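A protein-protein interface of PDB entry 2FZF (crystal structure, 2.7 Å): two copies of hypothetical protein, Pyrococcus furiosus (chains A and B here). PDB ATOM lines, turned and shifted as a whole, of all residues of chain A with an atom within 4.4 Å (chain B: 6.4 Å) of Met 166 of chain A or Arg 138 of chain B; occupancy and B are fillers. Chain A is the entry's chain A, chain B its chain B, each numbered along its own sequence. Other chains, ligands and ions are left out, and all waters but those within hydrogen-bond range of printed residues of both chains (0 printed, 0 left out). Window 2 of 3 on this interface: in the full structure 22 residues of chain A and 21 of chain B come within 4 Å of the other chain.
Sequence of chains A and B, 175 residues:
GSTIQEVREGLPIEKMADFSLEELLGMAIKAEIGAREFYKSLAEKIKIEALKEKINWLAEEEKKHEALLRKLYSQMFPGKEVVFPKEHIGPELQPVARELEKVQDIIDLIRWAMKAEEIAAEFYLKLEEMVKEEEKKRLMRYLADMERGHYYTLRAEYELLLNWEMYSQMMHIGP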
ATOM      1  N   GLU A 159      -9.009  -3.714  19.163  1.00  0.00           N
ATOM      2  CA  GLU A 159      -8.479  -5.044  19.469  1.00  0.00           C
ATOM      3  C   GLU A 159      -9.613  -6.060  19.687  1.00  0.00           C
ATOM      4  O   GLU A 159      -9.587  -7.156  19.136  1.00  0.00           O
ATOM      5  CB  GLU A 159      -7.601  -4.947  20.731  1.00  0.00           C
ATOM      6  CG  GLU A 159      -6.483  -5.981  20.863  1.00  0.00           C
ATOM      7  CD  GLU A 159      -5.440  -5.890  19.760  1.00  0.00           C
ATOM      8  OE1 GLU A 159      -5.724  -6.359  18.637  1.00  0.00           O
ATOM      9  OE2 GLU A 159      -4.347  -5.350  20.016  1.00  0.00           O
ATOM     10  N   LEU A 162     -11.956  -7.054  16.693  1.00  0.00           N
ATOM     11  CA  LEU A 162     -11.388  -7.991  15.726  1.00  0.00           C
ATOM     12  C   LEU A 162     -11.921  -9.402  15.930  1.00  0.00           C
ATOM     13  O   LEU A 162     -11.994 -10.197  14.986  1.00  0.00           O
ATOM     14  CB  LEU A 162      -9.867  -7.992  15.846  1.00  0.00           C
ATOM     15  CG  LEU A 162      -9.177  -6.704  15.406  1.00  0.00           C
ATOM     16  CD1 LEU A 162      -7.789  -6.668  16.013  1.00  0.00           C
ATOM     17  CD2 LEU A 162      -9.128  -6.609  13.878  1.00  0.00           C
ATOM     18  N   ASN A 163     -12.280  -9.710  17.173  1.00  0.00           N
ATOM     19  CA  ASN A 163     -12.825 -11.021  17.518  1.00  0.00           C
ATOM     20  C   ASN A 163     -14.219 -11.164  16.891  1.00  0.00           C
ATOM     21  O   ASN A 163     -14.646 -12.264  16.540  1.00  0.00           O
ATOM     22  CB  ASN A 163     -12.925 -11.167  19.048  1.00  0.00           C
ATOM     23  CG  ASN A 163     -11.562 -11.119  19.743  1.00  0.00           C
ATOM     24  OD1 ASN A 163     -10.713 -11.998  19.545  1.00  0.00           O
ATOM     25  ND2 ASN A 163     -11.352 -10.088  20.565  1.00  0.00           N
ATOM     26  N   GLU A 165     -15.620 -10.488  13.874  1.00  0.00           N
ATOM     27  CA  GLU A 165     -15.725 -11.243  12.634  1.00  0.00           C
ATOM     28  C   GLU A 165     -14.555 -12.197  12.421  1.00  0.00           C
ATOM     29  O   GLU A 165     -14.520 -13.289  12.989  1.00  0.00           O
ATOM     30  CB  GLU A 165     -15.845 -10.304  11.428  1.00  0.00           C
ATOM     31  CG  GLU A 165     -17.192  -9.621  11.276  1.00  0.00           C
ATOM     32  CD  GLU A 165     -17.352  -8.976   9.904  1.00  0.00           C
ATOM     33  OE1 GLU A 165     -16.467  -8.187   9.508  1.00  0.00           O
ATOM     34  OE2 GLU A 165     -18.361  -9.258   9.223  1.00  0.00           O
ATOM     35  N   MET A 166     -13.598 -11.776  11.600  1.00  0.00           N
ATOM     36  CA  MET A 166     -12.427 -12.590  11.272  1.00  0.00           C
ATOM     37  C   MET A 166     -12.802 -13.975  10.742  1.00  0.00           C
ATOM     38  O   MET A 166     -13.959 -14.235  10.410  1.00  0.00           O
ATOM     39  CB  MET A 166     -11.494 -12.712  12.483  1.00  0.00           C
ATOM     40  CG  MET A 166     -10.624 -11.469  12.719  1.00  0.00           C
ATOM     41  SD  MET A 166      -9.568 -10.979  11.297  1.00  0.00           S
ATOM     42  CE  MET A 166     -10.596  -9.722  10.516  1.00  0.00           C
ATOM     43  N   TYR A 167     -11.816 -14.861  10.654  1.00  0.00           N
ATOM     44  CA  TYR A 167     -12.060 -16.203  10.134  1.00  0.00           C
ATOM     45  C   TYR A 167     -11.340 -17.273  10.965  1.00  0.00           C
ATOM     46  O   TYR A 167     -10.807 -16.932  12.043  1.00  0.00           O
ATOM     47  CB  TYR A 167     -11.606 -16.279   8.663  1.00  0.00           C
ATOM     48  CG  TYR A 167     -11.757 -14.977   7.886  1.00  0.00           C
ATOM     49  CD1 TYR A 167     -10.856 -13.923   8.075  1.00  0.00           C
ATOM     50  CD2 TYR A 167     -12.808 -14.789   6.983  1.00  0.00           C
ATOM     51  CE1 TYR A 167     -10.996 -12.716   7.390  1.00  0.00           C
ATOM     52  CE2 TYR A 167     -12.959 -13.582   6.289  1.00  0.00           C
ATOM     53  CZ  TYR A 167     -12.049 -12.549   6.499  1.00  0.00           C
ATOM     54  OH  TYR A 167     -12.189 -11.346   5.835  1.00  0.00           O
ATOM     55  N   GLU B 128      -0.011 -12.566  27.603  1.00  0.00           N
ATOM     56  CA  GLU B 128      -0.372 -12.699  26.200  1.00  0.00           C
ATOM     57  C   GLU B 128       0.536 -13.740  25.582  1.00  0.00           C
ATOM     58  O   GLU B 128       0.131 -14.491  24.702  1.00  0.00           O
ATOM     59  CB  GLU B 128      -0.157 -11.380  25.461  1.00  0.00           C
ATOM     60  CG  GLU B 128      -0.728 -11.370  24.041  1.00  0.00           C
ATOM     61  CD  GLU B 128       0.069 -10.526  23.054  1.00  0.00           C
ATOM     62  OE1 GLU B 128       0.550  -9.434  23.427  1.00  0.00           O
ATOM     63  OE2 GLU B 128       0.196 -10.953  21.883  1.00  0.00           O
ATOM     64  N   GLU B 133      -3.897 -19.489  20.976  1.00  0.00           N
ATOM     65  CA  GLU B 133      -5.210 -19.198  20.401  1.00  0.00           C
ATOM     66  C   GLU B 133      -5.399 -17.684  20.307  1.00  0.00           C
ATOM     67  O   GLU B 133      -5.634 -17.012  21.306  1.00  0.00           O
ATOM     68  CB  GLU B 133      -6.313 -19.828  21.265  1.00  0.00           C
ATOM     69  CG  GLU B 133      -7.695 -19.847  20.612  1.00  0.00           C
ATOM     70  CD  GLU B 133      -8.701 -20.708  21.371  1.00  0.00           C
ATOM     71  OE1 GLU B 133      -8.361 -21.866  21.710  1.00  0.00           O
ATOM     72  OE2 GLU B 133      -9.835 -20.233  21.616  1.00  0.00           O
ATOM     73  N   GLU B 134      -5.293 -17.158  19.092  1.00  0.00           N
ATOM     74  CA  GLU B 134      -5.409 -15.726  18.847  1.00  0.00           C
ATOM     75  C   GLU B 134      -6.531 -14.952  19.539  1.00  0.00           C
ATOM     76  O   GLU B 134      -6.378 -13.754  19.795  1.00  0.00           O
ATOM     77  CB  GLU B 134      -5.462 -15.461  17.341  1.00  0.00           C
ATOM     78  CG  GLU B 134      -4.103 -15.581  16.658  1.00  0.00           C
ATOM     79  CD  GLU B 134      -3.177 -14.410  16.963  1.00  0.00           C
ATOM     80  OE1 GLU B 134      -1.957 -14.528  16.693  1.00  0.00           O
ATOM     81  OE2 GLU B 134      -3.663 -13.366  17.460  1.00  0.00           O
ATOM     82  N   GLU B 135      -7.649 -15.606  19.845  1.00  0.00           N
ATOM     83  CA  GLU B 135      -8.755 -14.908  20.507  1.00  0.00           C
ATOM     84  C   GLU B 135      -8.397 -14.484  21.935  1.00  0.00           C
ATOM     85  O   GLU B 135      -8.718 -13.370  22.361  1.00  0.00           O
ATOM     86  CB  GLU B 135     -10.024 -15.775  20.519  1.00  0.00           C
ATOM     87  CG  GLU B 135     -11.151 -15.164  21.361  1.00  0.00           C
ATOM     88  CD  GLU B 135     -12.476 -15.910  21.270  1.00  0.00           C
ATOM     89  OE1 GLU B 135     -13.324 -15.694  22.167  1.00  0.00           O
ATOM     90  OE2 GLU B 135     -12.677 -16.693  20.311  1.00  0.00           O
ATOM     91  N   LYS B 136      -7.737 -15.378  22.665  1.00  0.00           N
ATOM     92  CA  LYS B 136      -7.313 -15.107  24.033  1.00  0.00           C
ATOM     93  C   LYS B 136      -6.155 -14.112  24.031  1.00  0.00           C
ATOM     94  O   LYS B 136      -5.919 -13.415  25.013  1.00  0.00           O
ATOM     95  CB  LYS B 136      -6.894 -16.406  24.728  1.00  0.00           C
ATOM     96  CG  LYS B 136      -8.052 -17.245  25.244  1.00  0.00           C
ATOM     97  CD  LYS B 136      -9.144 -17.472  24.192  1.00  0.00           C
ATOM     98  CE  LYS B 136     -10.349 -18.225  24.792  1.00  0.00           C
ATOM     99  NZ  LYS B 136     -11.474 -18.484  23.831  1.00  0.00           N
ATOM    100  N   LYS B 137      -5.426 -14.041  22.924  1.00  0.00           N
ATOM    101  CA  LYS B 137      -4.324 -13.099  22.841  1.00  0.00           C
ATOM    102  C   LYS B 137      -4.867 -11.682  22.739  1.00  0.00           C
ATOM    103  O   LYS B 137      -4.339 -10.770  23.375  1.00  0.00           O
ATOM    104  CB  LYS B 137      -3.433 -13.415  21.637  1.00  0.00           C
ATOM    105  CG  LYS B 137      -2.638 -14.709  21.774  1.00  0.00           C
ATOM    106  CD  LYS B 137      -1.696 -14.890  20.598  1.00  0.00           C
ATOM    107  CE  LYS B 137      -0.626 -15.928  20.900  1.00  0.00           C
ATOM    108  NZ  LYS B 137       0.276 -15.516  22.014  1.00  0.00           N
ATOM    109  N   ARG B 138      -5.919 -11.495  21.940  1.00  0.00           N
ATOM    110  CA  ARG B 138      -6.535 -10.169  21.787  1.00  0.00           C
ATOM    111  C   ARG B 138      -7.025  -9.693  23.144  1.00  0.00           C
ATOM    112  O   ARG B 138      -6.808  -8.542  23.527  1.00  0.00           O
ATOM    113  CB  ARG B 138      -7.737 -10.214  20.829  1.00  0.00           C
ATOM    114  CG  ARG B 138      -7.416 -10.487  19.362  1.00  0.00           C
ATOM    115  CD  ARG B 138      -8.667 -10.272  18.512  1.00  0.00           C
ATOM    116  NE  ARG B 138      -8.594 -10.831  17.158  1.00  0.00           N
ATOM    117  CZ  ARG B 138      -7.644 -10.549  16.268  1.00  0.00           C
ATOM    118  NH1 ARG B 138      -6.654  -9.713  16.572  1.00  0.00           N
ATOM    119  NH2 ARG B 138      -7.707 -11.086  15.059  1.00  0.00           N
ATOM    120  N   LEU B 139      -7.695 -10.601  23.852  1.00  0.00           N
ATOM    121  CA  LEU B 139      -8.245 -10.344  25.178  1.00  0.00           C
ATOM    122  C   LEU B 139      -7.174  -9.784  26.113  1.00  0.00           C
ATOM    123  O   LEU B 139      -7.376  -8.759  26.756  1.00  0.00           O
ATOM    124  CB  LEU B 139      -8.809 -11.649  25.753  1.00  0.00           C
ATOM    125  CG  LEU B 139     -10.275 -11.680  26.191  1.00  0.00           C
ATOM    126  CD1 LEU B 139     -10.463 -10.847  27.464  1.00  0.00           C
ATOM    127  CD2 LEU B 139     -11.153 -11.161  25.041  1.00  0.00           C
ATOM    128  N   MET B 140      -6.038 -10.465  26.191  1.00  0.00           N
ATOM    129  CA  MET B 140      -4.973 -10.002  27.052  1.00  0.00           C
ATOM    130  C   MET B 140      -4.489  -8.668  26.487  1.00  0.00           C
ATOM    131  O   MET B 140      -4.197  -7.725  27.231  1.00  0.00           O
ATOM    132  CB  MET B 140      -3.823 -11.009  27.087  1.00  0.00           C
ATOM    133  CG  MET B 140      -4.241 -12.458  27.399  1.00  0.00           C
ATOM    134  SD  MET B 140      -5.099 -12.690  28.989  1.00  0.00           S
ATOM    135  CE  MET B 140      -4.150 -11.662  29.998  1.00  0.00           C
ATOM    136  N   ARG B 141      -4.423  -8.583  25.162  1.00  0.00           N
ATOM    137  CA  ARG B 141      -3.992  -7.351  24.527  1.00  0.00           C
ATOM    138  C   ARG B 141      -4.938  -6.209  24.900  1.00  0.00           C
ATOM    139  O   ARG B 141      -4.504  -5.084  25.192  1.00  0.00           O
ATOM    140  CB  ARG B 141      -3.901  -7.534  23.012  1.00  0.00           C
ATOM    141  CG  ARG B 141      -2.475  -7.345  22.528  1.00  0.00           C
ATOM    142  CD  ARG B 141      -2.339  -7.588  21.050  1.00  0.00           C
ATOM    143  NE  ARG B 141      -2.253  -9.012  20.739  1.00  0.00           N
ATOM    144  CZ  ARG B 141      -2.962  -9.603  19.786  1.00  0.00           C
ATOM    145  NH1 ARG B 141      -3.809  -8.890  19.060  1.00  0.00           N
ATOM    146  NH2 ARG B 141      -2.821 -10.898  19.563  1.00  0.00           N
ATOM    147  N   TYR B 142      -6.232  -6.503  24.911  1.00  0.00           N
ATOM    148  CA  TYR B 142      -7.229  -5.510  25.292  1.00  0.00           C
ATOM    149  C   TYR B 142      -6.922  -5.003  26.712  1.00  0.00           C
ATOM    150  O   TYR B 142      -6.755  -3.797  26.917  1.00  0.00           O
ATOM    151  CB  TYR B 142      -8.639  -6.133  25.209  1.00  0.00           C
ATOM    152  CG  TYR B 142      -9.698  -5.390  26.000  1.00  0.00           C
ATOM    153  CD1 TYR B 142      -9.991  -5.744  27.318  1.00  0.00           C
ATOM    154  CD2 TYR B 142     -10.350  -4.284  25.461  1.00  0.00           C
ATOM    155  CE1 TYR B 142     -10.903  -5.008  28.077  1.00  0.00           C
ATOM    156  CE2 TYR B 142     -11.258  -3.544  26.212  1.00  0.00           C
ATOM    157  CZ  TYR B 142     -11.528  -3.907  27.516  1.00  0.00           C
ATOM    158  OH  TYR B 142     -12.402  -3.147  28.255  1.00  0.00           O
ATOM    159  N   LEU B 143      -6.814  -5.931  27.668  1.00  0.00           N
ATOM    160  CA  LEU B 143      -6.534  -5.599  29.068  1.00  0.00           C
ATOM    161  C   LEU B 143      -5.237  -4.808  29.242  1.00  0.00           C
ATOM    162  O   LEU B 143      -5.137  -3.930  30.099  1.00  0.00           O
ATOM    163  CB  LEU B 143      -6.471  -6.875  29.918  1.00  0.00           C
ATOM    164  CG  LEU B 143      -7.713  -7.785  29.959  1.00  0.00           C
ATOM    165  CD1 LEU B 143      -7.332  -9.132  30.558  1.00  0.00           C
ATOM    166  CD2 LEU B 143      -8.824  -7.141  30.764  1.00  0.00           C
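Of the 6 printed residues of chain A, 4 touch a printed residue of chain B. Printed residues of chain A that touch a printed residue of chain B: Glu 159, Leu 162, Asn 163 and Met 166. Hydrophobic or aromatic side chains of chain A within 4 Å of the printed part of chain B: Leu 162 and Met 166. Among the printed residues, 6 pairs touch across the chains.
Glu 159 of chain A touches Arg 138 of chain B. Leu 162 of chain A touches Arg 138 of chain B (CD1 to NH1, 3.3 Å). Glu 135 of chain B touches Asn 163 of chain A (CA to OD1, 3.6 Å). Arg 138 of chain B touches Met 166 of chain A.
Of chain B, only Arg 138 comes within 4 Å of Met 166 of chain A. Of the printed residues of chain B, Asn 163 of chain A touches Glu 135 (3.6 Å) and Arg 138 (2.9 Å). Of the printed residues of chain A, Glu 135 of chain B touches Asn 163 (3.6 Å). Of the printed residues of chain B, Glu 159 of chain A touches Arg 138 and Arg 141. Of the printed residues of chain A, Arg 141 of chain B touches Glu 159. Glu 133 of chain B touches none of the printed residues of chain A. The nearest printed residue of chain A that does not touch Arg 138 of chain B is Tyr 167 of chain A (7.1 Å).
NE of Arg 141 of chain B lies within salt-bridge range of OE2 of Glu 128 of chain B (3.3 Å). The guanidinium group of Arg 141 of chain B lies within salt-bridge range of the side-chain carboxylate of Glu 134 of chain B, at 3.4 Å. OE1 of Glu 135 of chain B is in salt-bridge range of NZ of Lys 136 of chain B (3.7 Å).
No position is printed for both chains. Of the 6 pairs that touch across the chains among the printed residues, none has its exchanged pair printed and touching as well.
The side-chain carboxylate (OE1) of Glu 159 of chain A lies within salt-bridge range of the guanidinium group (NH1) of Arg 141 of chain B (3.2 Å). The side-chain amide oxygen of Asn 163 of chain A lies close to the guanidinium group of Arg 138 of chain B.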
